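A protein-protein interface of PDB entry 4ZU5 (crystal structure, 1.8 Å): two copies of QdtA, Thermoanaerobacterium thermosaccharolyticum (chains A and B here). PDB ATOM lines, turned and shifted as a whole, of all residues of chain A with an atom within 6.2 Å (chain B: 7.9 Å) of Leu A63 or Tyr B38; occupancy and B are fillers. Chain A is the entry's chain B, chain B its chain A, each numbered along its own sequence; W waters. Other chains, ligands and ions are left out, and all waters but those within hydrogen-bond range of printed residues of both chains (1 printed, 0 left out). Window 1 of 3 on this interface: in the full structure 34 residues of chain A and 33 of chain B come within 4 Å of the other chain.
The backbone carbonyl oxygen (O) of Val B36 lies within hydrogen-bond range of the backbone NH (N) of Ile A23, at 2.8 Å. The backbone carbonyl oxygen (O) of Thr B40 sits at hydrogen-bond distance from the backbone NH (N) of His A19 (2.9 Å). ND2 of Asn A64 sits close to ND2 of Asn B64, at 3.3 Å. The side-chain hydroxyl of Tyr B38 sits at hydrogen-bond distance from the backbone carbonyl oxygen of Pro A85 (2.7 Å). The backbone NH (N) of Tyr B38 is in hydrogen-bond range of the backbone carbonyl oxygen (O) of Thr A21 (3.0 Å).
The backbone carbonyl oxygen (O) of Asn B64 sits close to the side-chain sulfur (SG) of Cys B106, at 3.6 Å. The backbone carbonyl oxygen (O) of Gly B105 lies within hydrogen-bond range of the side-chain amide nitrogen (ND2) of Asn B64 (2.9 Å). OG1 of Thr B40 lies within hydrogen-bond range of NZ of Lys B41, 2.8 Å away. The backbone NH of Phe A10 is in hydrogen-bond range of the backbone carbonyl oxygen of Ser A86. O of Val B107 lies within hydrogen-bond range of N of Leu B63. The backbone NH of Val B107 is in hydrogen-bond range of the backbone carbonyl oxygen of Asn B64 (3.2 Å).
O of His A19 touches O of Tyr B38 (3.8 Å). CD2 of His A19 touches CB of Lys B41 (3.7 Å). Tyr B37 touches Leu A20. Thr A21 touches Tyr B37. Val B36 touches Pro A22. Tyr B38 touches Ile A23 (OH to CD1, 3.6 Å). CG2 of Ile A61 touches OH of Tyr B38, 3.5 Å away. NZ of Lys B41 touches CG of Pro A85, at 3.8 Å. Leu B63 touches Val A107 (O to CG2, 3.9 Å). CG2 of Val A107 touches CB of Asn B64, at 3.7 Å.
Of the printed residues of chain B, Leu A63 touches Tyr B38, Thr B40 and Val B107. Tyr B38 touches just these residues of chain A: Phe A10 (3.9 Å), His A19 (3.8 Å), Leu A20 (3.2 Å), Thr A21 (3.0 Å), Ile A23 (3.6 Å), Ile A61 (3.5 Å), Leu A63 (3.3 Å) and Pro A85 (2.7 Å). No residue of chain B comes within 4 Å of Cys A62. Printed residues of chain A within 4 Å of Leu B63: Val A107. Of the printed residues of chain A, Ile B39 touches His A19 and Leu A20. Of the printed residues of chain B, Asn A64 touches Asn B64 (3.3 Å), Gly B105 (3.8 Å) and Val B107 (3.8 Å). Asp A84 touches none of the printed residues of chain B. The nearest printed residue of chain B that does not touch Asn A64 is Cys B106 (5.6 Å).
Hydrophobic or aromatic side chains of chain A within 4 Å of the printed part of chain B: Phe A10, His A19, Leu A20, Ile A23, Ile A61, Leu A63, Pro A85 and Val A107. Among the printed residues, 26 pairs touch across the chains.
Leu A63 touches Val B107, and with the chains exchanged Val A107 touches Leu B63. Asn B64 touches its own counterpart, Asn A64. Asn A64 touches Val B107, and with the chains exchanged Val A107 touches Asn B64.
Water W1 lies within hydrogen-bond range of the side-chain hydroxyl (OG1) of Thr B40, the backbone carbonyl oxygen (O) of His A19 and the backbone carbonyl oxygen (O) of Tyr B38.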
ATOM      1  N   PHE A  10     -27.703  13.217 -29.084  1.00  0.00           N
ATOM      2  CA  PHE A  10     -28.410  14.442 -28.700  1.00  0.00           C
ATOM      3  C   PHE A  10     -28.827  15.283 -29.902  1.00  0.00           C
ATOM      4  O   PHE A  10     -28.179  15.237 -30.935  1.00  0.00           O
ATOM      5  CB  PHE A  10     -27.555  15.284 -27.705  1.00  0.00           C
ATOM      6  CG  PHE A  10     -27.069  14.491 -26.517  1.00  0.00           C
ATOM      7  CD1 PHE A  10     -25.720  14.370 -26.245  1.00  0.00           C
ATOM      8  CD2 PHE A  10     -27.963  13.913 -25.648  1.00  0.00           C
ATOM      9  CE1 PHE A  10     -25.283  13.652 -25.138  1.00  0.00           C
ATOM     10  CE2 PHE A  10     -27.552  13.237 -24.511  1.00  0.00           C
ATOM     11  CZ  PHE A  10     -26.202  13.088 -24.264  1.00  0.00           C
ATOM     12  N   HIS A  19     -23.433  26.001 -33.300  1.00  0.00           N
ATOM     13  CA  HIS A  19     -24.117  24.803 -32.858  1.00  0.00           C
ATOM     14  C   HIS A  19     -24.456  24.842 -31.373  1.00  0.00           C
ATOM     15  O   HIS A  19     -23.640  25.268 -30.569  1.00  0.00           O
ATOM     16  CB  HIS A  19     -23.162  23.655 -33.053  1.00  0.00           C
ATOM     17  CG  HIS A  19     -22.940  23.301 -34.484  1.00  0.00           C
ATOM     18  ND1 HIS A  19     -23.417  22.131 -35.029  1.00  0.00           N
ATOM     19  CD2 HIS A  19     -22.222  23.911 -35.454  1.00  0.00           C
ATOM     20  CE1 HIS A  19     -23.007  22.034 -36.281  1.00  0.00           C
ATOM     21  NE2 HIS A  19     -22.296  23.109 -36.570  1.00  0.00           N
ATOM     22  N   LEU A  20     -25.601  24.286 -31.013  1.00  0.00           N
ATOM     23  CA  LEU A  20     -26.027  24.184 -29.621  1.00  0.00           C
ATOM     24  C   LEU A  20     -26.627  22.786 -29.404  1.00  0.00           C
ATOM     25  O   LEU A  20     -27.433  22.298 -30.240  1.00  0.00           O
ATOM     26  CB  LEU A  20     -27.050  25.281 -29.278  1.00  0.00           C
ATOM     27  CG  LEU A  20     -27.602  25.392 -27.847  1.00  0.00           C
ATOM     28  CD1 LEU A  20     -28.041  26.800 -27.548  1.00  0.00           C
ATOM     29  CD2 LEU A  20     -28.788  24.478 -27.581  1.00  0.00           C
ATOM     30  N   THR A  21     -26.196  22.127 -28.319  1.00  0.00           N
ATOM     31  CA  THR A  21     -26.838  20.885 -27.883  1.00  0.00           C
ATOM     32  C   THR A  21     -27.391  21.026 -26.482  1.00  0.00           C
ATOM     33  O   THR A  21     -26.635  21.444 -25.580  1.00  0.00           O
ATOM     34  CB  THR A  21     -25.830  19.752 -27.952  1.00  0.00           C
ATOM     35  OG1 THR A  21     -25.689  19.368 -29.321  1.00  0.00           O
ATOM     36  CG2 THR A  21     -26.259  18.536 -27.156  1.00  0.00           C
ATOM     37  N   PRO A  22     -28.689  20.711 -26.299  1.00  0.00           N
ATOM     38  CA  PRO A  22     -29.277  20.710 -24.989  1.00  0.00           C
ATOM     39  C   PRO A  22     -29.458  19.303 -24.440  1.00  0.00           C
ATOM     40  O   PRO A  22     -29.708  18.352 -25.182  1.00  0.00           O
ATOM     41  CB  PRO A  22     -30.642  21.338 -25.235  1.00  0.00           C
ATOM     42  CG  PRO A  22     -31.023  20.717 -26.537  1.00  0.00           C
ATOM     43  CD  PRO A  22     -29.744  20.495 -27.302  1.00  0.00           C
ATOM     44  N   ILE A  23     -29.345  19.198 -23.129  1.00  0.00           N
ATOM     45  CA  ILE A  23     -29.509  17.896 -22.453  1.00  0.00           C
ATOM     46  C   ILE A  23     -30.333  18.206 -21.219  1.00  0.00           C
ATOM     47  O   ILE A  23     -29.851  18.849 -20.319  1.00  0.00           O
ATOM     48  CB  ILE A  23     -28.165  17.250 -22.062  1.00  0.00           C
ATOM     49  CG1 ILE A  23     -27.213  17.136 -23.247  1.00  0.00           C
ATOM     50  CG2 ILE A  23     -28.366  15.922 -21.366  1.00  0.00           C
ATOM     51  CD1 ILE A  23     -25.817  16.708 -22.903  1.00  0.00           C
ATOM     52  N   ILE A  61     -19.005  13.241 -22.636  1.00  0.00           N
ATOM     53  CA  ILE A  61     -19.198  13.937 -23.896  1.00  0.00           C
ATOM     54  C   ILE A  61     -17.986  14.789 -24.216  1.00  0.00           C
ATOM     55  O   ILE A  61     -17.514  15.556 -23.390  1.00  0.00           O
ATOM     56  CB  ILE A  61     -20.430  14.850 -23.848  1.00  0.00           C
ATOM     57  CG1 ILE A  61     -21.649  14.159 -23.229  1.00  0.00           C
ATOM     58  CG2 ILE A  61     -20.684  15.473 -25.195  1.00  0.00           C
ATOM     59  CD1 ILE A  61     -22.426  15.107 -22.372  1.00  0.00           C
ATOM     60  N   CYS A  62     -17.424  14.585 -25.401  1.00  0.00           N
ATOM     61  CA  CYS A  62     -16.301  15.375 -25.831  1.00  0.00           C
ATOM     62  C   CYS A  62     -16.822  16.607 -26.599  1.00  0.00           C
ATOM     63  O   CYS A  62     -17.366  16.521 -27.696  1.00  0.00           O
ATOM     64  CB  CYS A  62     -15.319  14.545 -26.660  1.00  0.00           C
ATOM     65  SG  CYS A  62     -13.866  15.540 -27.087  1.00  0.00           S
ATOM     66  N   LEU A  63     -16.587  17.789 -26.032  1.00  0.00           N
ATOM     67  CA  LEU A  63     -17.166  19.018 -26.548  1.00  0.00           C
ATOM     68  C   LEU A  63     -16.211  19.768 -27.478  1.00  0.00           C
ATOM     69  O   LEU A  63     -16.624  20.708 -28.172  1.00  0.00           O
ATOM     70  CB  LEU A  63     -17.501  19.901 -25.360  1.00  0.00           C
ATOM     71  CG  LEU A  63     -18.482  19.339 -24.317  1.00  0.00           C
ATOM     72  CD1 LEU A  63     -18.699  20.451 -23.305  1.00  0.00           C
ATOM     73  CD2 LEU A  63     -19.806  18.987 -24.955  1.00  0.00           C
ATOM     74  N   ASN A  64     -14.933  19.381 -27.447  1.00  0.00           N
ATOM     75  CA  ASN A  64     -13.929  19.920 -28.392  1.00  0.00           C
ATOM     76  C   ASN A  64     -12.788  18.950 -28.530  1.00  0.00           C
ATOM     77  O   ASN A  64     -12.360  18.325 -27.566  1.00  0.00           O
ATOM     78  CB  ASN A  64     -13.387  21.296 -27.972  1.00  0.00           C
ATOM     79  CG  ASN A  64     -12.571  21.955 -29.078  1.00  0.00           C
ATOM     80  OD1 ASN A  64     -13.053  22.127 -30.174  1.00  0.00           O
ATOM     81  ND2 ASN A  64     -11.385  22.376 -28.760  1.00  0.00           N
ATOM     82  N   GLY A  65     -12.312  18.781 -29.757  1.00  0.00           N
ATOM     83  CA  GLY A  65     -11.175  17.893 -29.981  1.00  0.00           C
ATOM     84  C   GLY A  65     -11.642  16.447 -29.942  1.00  0.00           C
ATOM     85  O   GLY A  65     -12.756  16.132 -30.389  1.00  0.00           O
ATOM     86  N   ASP A  84     -17.446  14.177 -31.039  1.00  0.00           N
ATOM     87  CA  ASP A  84     -18.617  14.861 -31.542  1.00  0.00           C
ATOM     88  C   ASP A  84     -19.467  15.300 -30.356  1.00  0.00           C
ATOM     89  O   ASP A  84     -19.916  14.434 -29.600  1.00  0.00           O
ATOM     90  CB  ASP A  84     -19.402  13.890 -32.410  1.00  0.00           C
ATOM     91  CG  ASP A  84     -20.691  14.449 -32.917  1.00  0.00           C
ATOM     92  OD1 ASP A  84     -21.245  15.496 -32.472  1.00  0.00           O
ATOM     93  OD2 ASP A  84     -21.240  13.757 -33.776  1.00  0.00           O
ATOM     94  N   PRO A  85     -19.736  16.602 -30.233  1.00  0.00           N
ATOM     95  CA  PRO A  85     -20.394  17.084 -29.026  1.00  0.00           C
ATOM     96  C   PRO A  85     -21.819  16.613 -28.909  1.00  0.00           C
ATOM     97  O   PRO A  85     -22.385  16.756 -27.860  1.00  0.00           O
ATOM     98  CB  PRO A  85     -20.341  18.601 -29.168  1.00  0.00           C
ATOM     99  CG  PRO A  85     -19.113  18.845 -29.986  1.00  0.00           C
ATOM    100  CD  PRO A  85     -19.097  17.701 -30.982  1.00  0.00           C
ATOM    101  N   SER A  86     -22.411  16.082 -29.973  1.00  0.00           N
ATOM    102  CA  SER A  86     -23.815  15.714 -29.995  1.00  0.00           C
ATOM    103  C   SER A  86     -24.035  14.239 -29.677  1.00  0.00           C
ATOM    104  O   SER A  86     -25.170  13.760 -29.743  1.00  0.00           O
ATOM    105  CB  SER A  86     -24.409  16.032 -31.359  1.00  0.00           C
ATOM    106  OG  SER A  86     -23.930  15.118 -32.344  1.00  0.00           O
ATOM    107  N   VAL A  87     -22.945  13.549 -29.347  1.00  0.00           N
ATOM    108  CA  VAL A  87     -22.946  12.176 -28.909  1.00  0.00           C
ATOM    109  C   VAL A  87     -22.371  11.986 -27.488  1.00  0.00           C
ATOM    110  O   VAL A  87     -21.271  12.414 -27.190  1.00  0.00           O
ATOM    111  CB  VAL A  87     -22.116  11.318 -29.851  1.00  0.00           C
ATOM    112  CG1 VAL A  87     -22.128   9.863 -29.359  1.00  0.00           C
ATOM    113  CG2 VAL A  87     -22.673  11.429 -31.264  1.00  0.00           C
ATOM    114  N   VAL A 107     -11.918  18.964 -24.523  1.00  0.00           N
ATOM    115  CA  VAL A 107     -12.771  19.237 -23.343  1.00  0.00           C
ATOM    116  C   VAL A 107     -13.652  17.995 -23.149  1.00  0.00           C
ATOM    117  O   VAL A 107     -14.391  17.663 -24.095  1.00  0.00           O
ATOM    118  CB  VAL A 107     -13.719  20.394 -23.617  1.00  0.00           C
ATOM    119  CG1 VAL A 107     -14.668  20.539 -22.437  1.00  0.00           C
ATOM    120  CG2 VAL A 107     -13.022  21.734 -23.897  1.00  0.00           C
ATOM    121  N   LEU A 108     -13.539  17.298 -22.024  1.00  0.00           N
ATOM    122  CA  LEU A 108     -14.429  16.172 -21.722  1.00  0.00           C
ATOM    123  C   LEU A 108     -15.374  16.552 -20.576  1.00  0.00           C
ATOM    124  O   LEU A 108     -14.928  16.841 -19.452  1.00  0.00           O
ATOM    125  CB  LEU A 108     -13.626  14.951 -21.335  1.00  0.00           C
ATOM    126  CG  LEU A 108     -14.430  13.695 -20.983  1.00  0.00           C
ATOM    127  CD1 LEU A 108     -15.219  13.208 -22.181  1.00  0.00           C
ATOM    128  CD2 LEU A 108     -13.447  12.659 -20.487  1.00  0.00           C
ATOM    129  N   LEU A 109     -16.668  16.515 -20.869  1.00  0.00           N
ATOM    130  CA  LEU A 109     -17.655  16.895 -19.873  1.00  0.00           C
ATOM    131  C   LEU A 109     -18.240  15.586 -19.383  1.00  0.00           C
ATOM    132  O   LEU A 109     -18.489  14.701 -20.185  1.00  0.00           O
ATOM    133  CB  LEU A 109     -18.743  17.727 -20.552  1.00  0.00           C
ATOM    134  CG  LEU A 109     -20.021  17.953 -19.748  1.00  0.00           C
ATOM    135  CD1 LEU A 109     -19.723  18.808 -18.527  1.00  0.00           C
ATOM    136  CD2 LEU A 109     -21.094  18.678 -20.529  1.00  0.00           C
ATOM    137  N   VAL B  36     -28.587  21.220 -19.039  1.00  0.00           N
ATOM    138  CA  VAL B  36     -27.355  21.831 -19.489  1.00  0.00           C
ATOM    139  C   VAL B  36     -27.462  21.974 -20.990  1.00  0.00           C
ATOM    140  O   VAL B  36     -28.256  21.301 -21.661  1.00  0.00           O
ATOM    141  CB  VAL B  36     -26.068  21.088 -19.130  1.00  0.00           C
ATOM    142  CG1 VAL B  36     -25.896  20.748 -17.658  1.00  0.00           C
ATOM    143  CG2 VAL B  36     -25.934  19.857 -19.971  1.00  0.00           C
ATOM    144  N   TYR B  37     -26.773  22.981 -21.502  1.00  0.00           N
ATOM    145  CA  TYR B  37     -26.536  23.047 -22.910  1.00  0.00           C
ATOM    146  C   TYR B  37     -25.222  23.669 -23.221  1.00  0.00           C
ATOM    147  O   TYR B  37     -24.622  24.338 -22.391  1.00  0.00           O
ATOM    148  CB  TYR B  37     -27.687  23.747 -23.636  1.00  0.00           C
ATOM    149  CG  TYR B  37     -27.939  25.191 -23.281  1.00  0.00           C
ATOM    150  CD1 TYR B  37     -27.308  26.185 -23.959  1.00  0.00           C
ATOM    151  CD2 TYR B  37     -28.818  25.556 -22.272  1.00  0.00           C
ATOM    152  CE1 TYR B  37     -27.530  27.515 -23.674  1.00  0.00           C
ATOM    153  CE2 TYR B  37     -29.061  26.893 -21.979  1.00  0.00           C
ATOM    154  CZ  TYR B  37     -28.429  27.865 -22.721  1.00  0.00           C
ATOM    155  OH  TYR B  37     -28.610  29.187 -22.450  1.00  0.00           O
ATOM    156  N   TYR B  38     -24.720  23.406 -24.418  1.00  0.00           N
ATOM    157  CA  TYR B  38     -23.422  23.967 -24.743  1.00  0.00           C
ATOM    158  C   TYR B  38     -23.373  24.446 -26.197  1.00  0.00           C
ATOM    159  O   TYR B  38     -24.062  23.851 -27.080  1.00  0.00           O
ATOM    160  CB  TYR B  38     -22.297  22.945 -24.490  1.00  0.00           C
ATOM    161  CG  TYR B  38     -22.673  21.513 -24.751  1.00  0.00           C
ATOM    162  CD1 TYR B  38     -22.448  20.939 -25.992  1.00  0.00           C
ATOM    163  CD2 TYR B  38     -23.131  20.676 -23.717  1.00  0.00           C
ATOM    164  CE1 TYR B  38     -22.789  19.624 -26.257  1.00  0.00           C
ATOM    165  CE2 TYR B  38     -23.439  19.343 -23.975  1.00  0.00           C
ATOM    166  CZ  TYR B  38     -23.271  18.830 -25.260  1.00  0.00           C
ATOM    167  OH  TYR B  38     -23.513  17.506 -25.578  1.00  0.00           O
ATOM    168  N   ILE B  39     -22.535  25.466 -26.429  1.00  0.00           N
ATOM    169  CA  ILE B  39     -22.425  26.143 -27.711  1.00  0.00           C
ATOM    170  C   ILE B  39     -21.006  25.990 -28.227  1.00  0.00           C
ATOM    171  O   ILE B  39     -20.026  26.241 -27.520  1.00  0.00           O
ATOM    172  CB  ILE B  39     -22.833  27.619 -27.576  1.00  0.00           C
ATOM    173  CG1 ILE B  39     -24.320  27.679 -27.226  1.00  0.00           C
ATOM    174  CG2 ILE B  39     -22.587  28.378 -28.871  1.00  0.00           C
ATOM    175  CD1 ILE B  39     -24.741  28.928 -26.505  1.00  0.00           C
ATOM    176  N   THR B  40     -20.900  25.493 -29.454  1.00  0.00           N
ATOM    177  CA  THR B  40     -19.614  25.260 -30.084  1.00  0.00           C
ATOM    178  C   THR B  40     -19.684  25.738 -31.558  1.00  0.00           C
ATOM    179  O   THR B  40     -20.746  26.045 -32.096  1.00  0.00           O
ATOM    180  CB  THR B  40     -19.284  23.757 -30.112  1.00  0.00           C
ATOM    181  OG1 THR B  40     -20.348  23.080 -30.814  1.00  0.00           O
ATOM    182  CG2 THR B  40     -19.150  23.192 -28.687  1.00  0.00           C
ATOM    183  N   LYS B  41     -18.504  25.894 -32.139  1.00  0.00           N
ATOM    184  CA  LYS B  41     -18.330  26.109 -33.568  1.00  0.00           C
ATOM    185  C   LYS B  41     -18.992  27.431 -33.985  1.00  0.00           C
ATOM    186  O   LYS B  41     -19.587  27.526 -35.048  1.00  0.00           O
ATOM    187  CB  LYS B  41     -18.787  24.858 -34.366  1.00  0.00           C
ATOM    188  CG  LYS B  41     -17.901  23.647 -34.103  1.00  0.00           C
ATOM    189  CD  LYS B  41     -18.246  22.383 -34.895  1.00  0.00           C
ATOM    190  CE  LYS B  41     -19.464  21.659 -34.310  1.00  0.00           C
ATOM    191  NZ  LYS B  41     -19.386  21.335 -32.835  1.00  0.00           N
ATOM    192  N   ARG B  48     -24.641  36.072 -30.600  1.00  0.00           N
ATOM    193  CA  ARG B  48     -25.890  35.340 -30.376  1.00  0.00           C
ATOM    194  C   ARG B  48     -26.453  35.682 -29.022  1.00  0.00           C
ATOM    195  O   ARG B  48     -25.916  36.562 -28.338  1.00  0.00           O
ATOM    196  CB  ARG B  48     -25.708  33.825 -30.515  1.00  0.00           C
ATOM    197  CG  ARG B  48     -24.534  33.252 -29.763  1.00  0.00           C
ATOM    198  CD  ARG B  48     -24.386  31.757 -30.046  1.00  0.00           C
ATOM    199  NE  ARG B  48     -25.619  31.060 -29.689  1.00  0.00           N
ATOM    200  CZ  ARG B  48     -26.121  30.013 -30.331  1.00  0.00           C
ATOM    201  NH1 ARG B  48     -27.267  29.525 -29.931  1.00  0.00           N
ATOM    202  NH2 ARG B  48     -25.492  29.439 -31.349  1.00  0.00           N
ATOM    203  N   ILE B  61     -20.193  29.057 -18.414  1.00  0.00           N
ATOM    204  CA  ILE B  61     -18.762  28.731 -18.221  1.00  0.00           C
ATOM    205  C   ILE B  61     -18.104  28.471 -19.561  1.00  0.00           C
ATOM    206  O   ILE B  61     -18.628  27.712 -20.381  1.00  0.00           O
ATOM    207  CB  ILE B  61     -18.565  27.437 -17.358  1.00  0.00           C
ATOM    208  CG1 ILE B  61     -19.504  27.440 -16.158  1.00  0.00           C
ATOM    209  CG2 ILE B  61     -17.111  27.247 -16.919  1.00  0.00           C
ATOM    210  CD1 ILE B  61     -19.973  26.064 -15.754  1.00  0.00           C
ATOM    211  N   LEU B  63     -15.289  26.685 -21.391  1.00  0.00           N
ATOM    212  CA  LEU B  63     -14.499  25.507 -21.054  1.00  0.00           C
ATOM    213  C   LEU B  63     -13.226  25.451 -21.910  1.00  0.00           C
ATOM    214  O   LEU B  63     -12.302  24.732 -21.590  1.00  0.00           O
ATOM    215  CB  LEU B  63     -15.316  24.210 -21.260  1.00  0.00           C
ATOM    216  CG  LEU B  63     -16.554  24.129 -20.348  1.00  0.00           C
ATOM    217  CD1 LEU B  63     -17.154  22.733 -20.387  1.00  0.00           C
ATOM    218  CD2 LEU B  63     -16.215  24.472 -18.919  1.00  0.00           C
ATOM    219  N   ASN B  64     -13.202  26.250 -22.969  1.00  0.00           N
ATOM    220  CA  ASN B  64     -12.047  26.299 -23.859  1.00  0.00           C
ATOM    221  C   ASN B  64     -12.152  27.596 -24.667  1.00  0.00           C
ATOM    222  O   ASN B  64     -13.253  28.050 -25.033  1.00  0.00           O
ATOM    223  CB  ASN B  64     -12.046  25.141 -24.839  1.00  0.00           C
ATOM    224  CG  ASN B  64     -10.731  25.045 -25.586  1.00  0.00           C
ATOM    225  OD1 ASN B  64      -9.637  25.009 -24.996  1.00  0.00           O
ATOM    226  ND2 ASN B  64     -10.840  25.037 -26.892  1.00  0.00           N
ATOM    227  N   PHE B 102     -16.558  34.758 -29.890  1.00  0.00           N
ATOM    228  CA  PHE B 102     -16.184  33.388 -29.640  1.00  0.00           C
ATOM    229  C   PHE B 102     -14.876  33.106 -30.381  1.00  0.00           C
ATOM    230  O   PHE B 102     -14.827  33.289 -31.590  1.00  0.00           O
ATOM    231  CB  PHE B 102     -17.276  32.483 -30.202  1.00  0.00           C
ATOM    232  CG  PHE B 102     -18.540  32.453 -29.417  1.00  0.00           C
ATOM    233  CD1 PHE B 102     -19.519  33.410 -29.589  1.00  0.00           C
ATOM    234  CD2 PHE B 102     -18.809  31.371 -28.561  1.00  0.00           C
ATOM    235  CE1 PHE B 102     -20.737  33.323 -28.912  1.00  0.00           C
ATOM    236  CE2 PHE B 102     -20.004  31.290 -27.862  1.00  0.00           C
ATOM    237  CZ  PHE B 102     -20.983  32.263 -28.046  1.00  0.00           C
ATOM    238  N   GLY B 105     -12.423  27.193 -31.537  1.00  0.00           N
ATOM    239  CA  GLY B 105     -12.377  26.116 -30.535  1.00  0.00           C
ATOM    240  C   GLY B 105     -13.184  26.434 -29.267  1.00  0.00           C
ATOM    241  O   GLY B 105     -13.243  25.622 -28.361  1.00  0.00           O
ATOM    242  N   CYS B 106     -13.829  27.599 -29.190  1.00  0.00           N
ATOM    243  CA  CYS B 106     -14.536  27.976 -27.950  1.00  0.00           C
ATOM    244  C   CYS B 106     -15.665  27.005 -27.633  1.00  0.00           C
ATOM    245  O   CYS B 106     -16.397  26.565 -28.518  1.00  0.00           O
ATOM    246  CB  CYS B 106     -15.142  29.353 -28.086  1.00  0.00           C
ATOM    247  SG  CYS B 106     -15.883  30.023 -26.567  1.00  0.00           S
ATOM    248  N   VAL B 107     -15.880  26.784 -26.346  1.00  0.00           N
ATOM    249  CA  VAL B 107     -16.968  25.950 -25.866  1.00  0.00           C
ATOM    250  C   VAL B 107     -17.588  26.691 -24.691  1.00  0.00           C
ATOM    251  O   VAL B 107     -16.876  26.953 -23.719  1.00  0.00           O
ATOM    252  CB  VAL B 107     -16.448  24.646 -25.260  1.00  0.00           C
ATOM    253  CG1 VAL B 107     -17.572  23.921 -24.584  1.00  0.00           C
ATOM    254  CG2 VAL B 107     -15.767  23.755 -26.287  1.00  0.00           C
ATOM    255  N   LEU B 108     -18.843  27.052 -24.820  1.00  0.00           N
ATOM    256  CA  LEU B 108     -19.591  27.732 -23.738  1.00  0.00           C
ATOM    257  C   LEU B 108     -20.613  26.714 -23.184  1.00  0.00           C
ATOM    258  O   LEU B 108     -21.474  26.246 -23.942  1.00  0.00           O
ATOM    259  CB  LEU B 108     -20.353  28.876 -24.363  1.00  0.00           C
ATOM    260  CG  LEU B 108     -21.155  29.765 -23.390  1.00  0.00           C
ATOM    261  CD1 LEU B 108     -20.321  30.178 -22.189  1.00  0.00           C
ATOM    262  CD2 LEU B 108     -21.826  30.972 -24.037  1.00  0.00           C
ATOM    263  N   LEU B 109     -20.537  26.436 -21.882  1.00  0.00           N
ATOM    264  CA  LEU B 109     -21.441  25.532 -21.200  1.00  0.00           C
ATOM    265  C   LEU B 109     -22.400  26.366 -20.362  1.00  0.00           C
ATOM    266  O   LEU B 109     -21.980  27.324 -19.716  1.00  0.00           O
ATOM    267  CB  LEU B 109     -20.646  24.635 -20.266  1.00  0.00           C
ATOM    268  CG  LEU B 109     -21.468  23.749 -19.348  1.00  0.00           C
ATOM    269  CD1 LEU B 109     -22.157  22.709 -20.232  1.00  0.00           C
ATOM    270  CD2 LEU B 109     -20.547  23.057 -18.359  1.00  0.00           C
ATOM    271  N   VAL B 110     -23.667  25.993 -20.367  1.00  0.00           N
ATOM    272  CA  VAL B 110     -24.635  26.668 -19.535  1.00  0.00           C
ATOM    273  C   VAL B 110     -25.313  25.617 -18.668  1.00  0.00           C
ATOM    274  O   VAL B 110     -25.758  24.613 -19.166  1.00  0.00           O
ATOM    275  CB  VAL B 110     -25.676  27.394 -20.404  1.00  0.00           C
ATOM    276  CG1 VAL B 110     -26.748  28.101 -19.559  1.00  0.00           C
ATOM    277  CG2 VAL B 110     -24.943  28.356 -21.367  1.00  0.00           C
ATOM    278  N   LEU B 111     -25.364  25.869 -17.366  1.00  0.00           N
ATOM    279  CA  LEU B 111     -26.149  25.100 -16.429  1.00  0.00           C
ATOM    280  C   LEU B 111     -27.400  25.904 -16.062  1.00  0.00           C
ATOM    281  O   LEU B 111     -27.314  27.093 -15.847  1.00  0.00           O
ATOM    282  CB  LEU B 111     -25.361  24.851 -15.148  1.00  0.00           C
ATOM    283  CG  LEU B 111     -23.904  24.444 -15.339  1.00  0.00           C
ATOM    284  CD1 LEU B 111     -23.156  24.347 -14.007  1.00  0.00           C
ATOM    285  CD2 LEU B 111     -23.756  23.194 -16.162  1.00  0.00           C
HETATM  286  O   HOH W   1     -22.467  22.474 -29.519  1.00  0.00           O
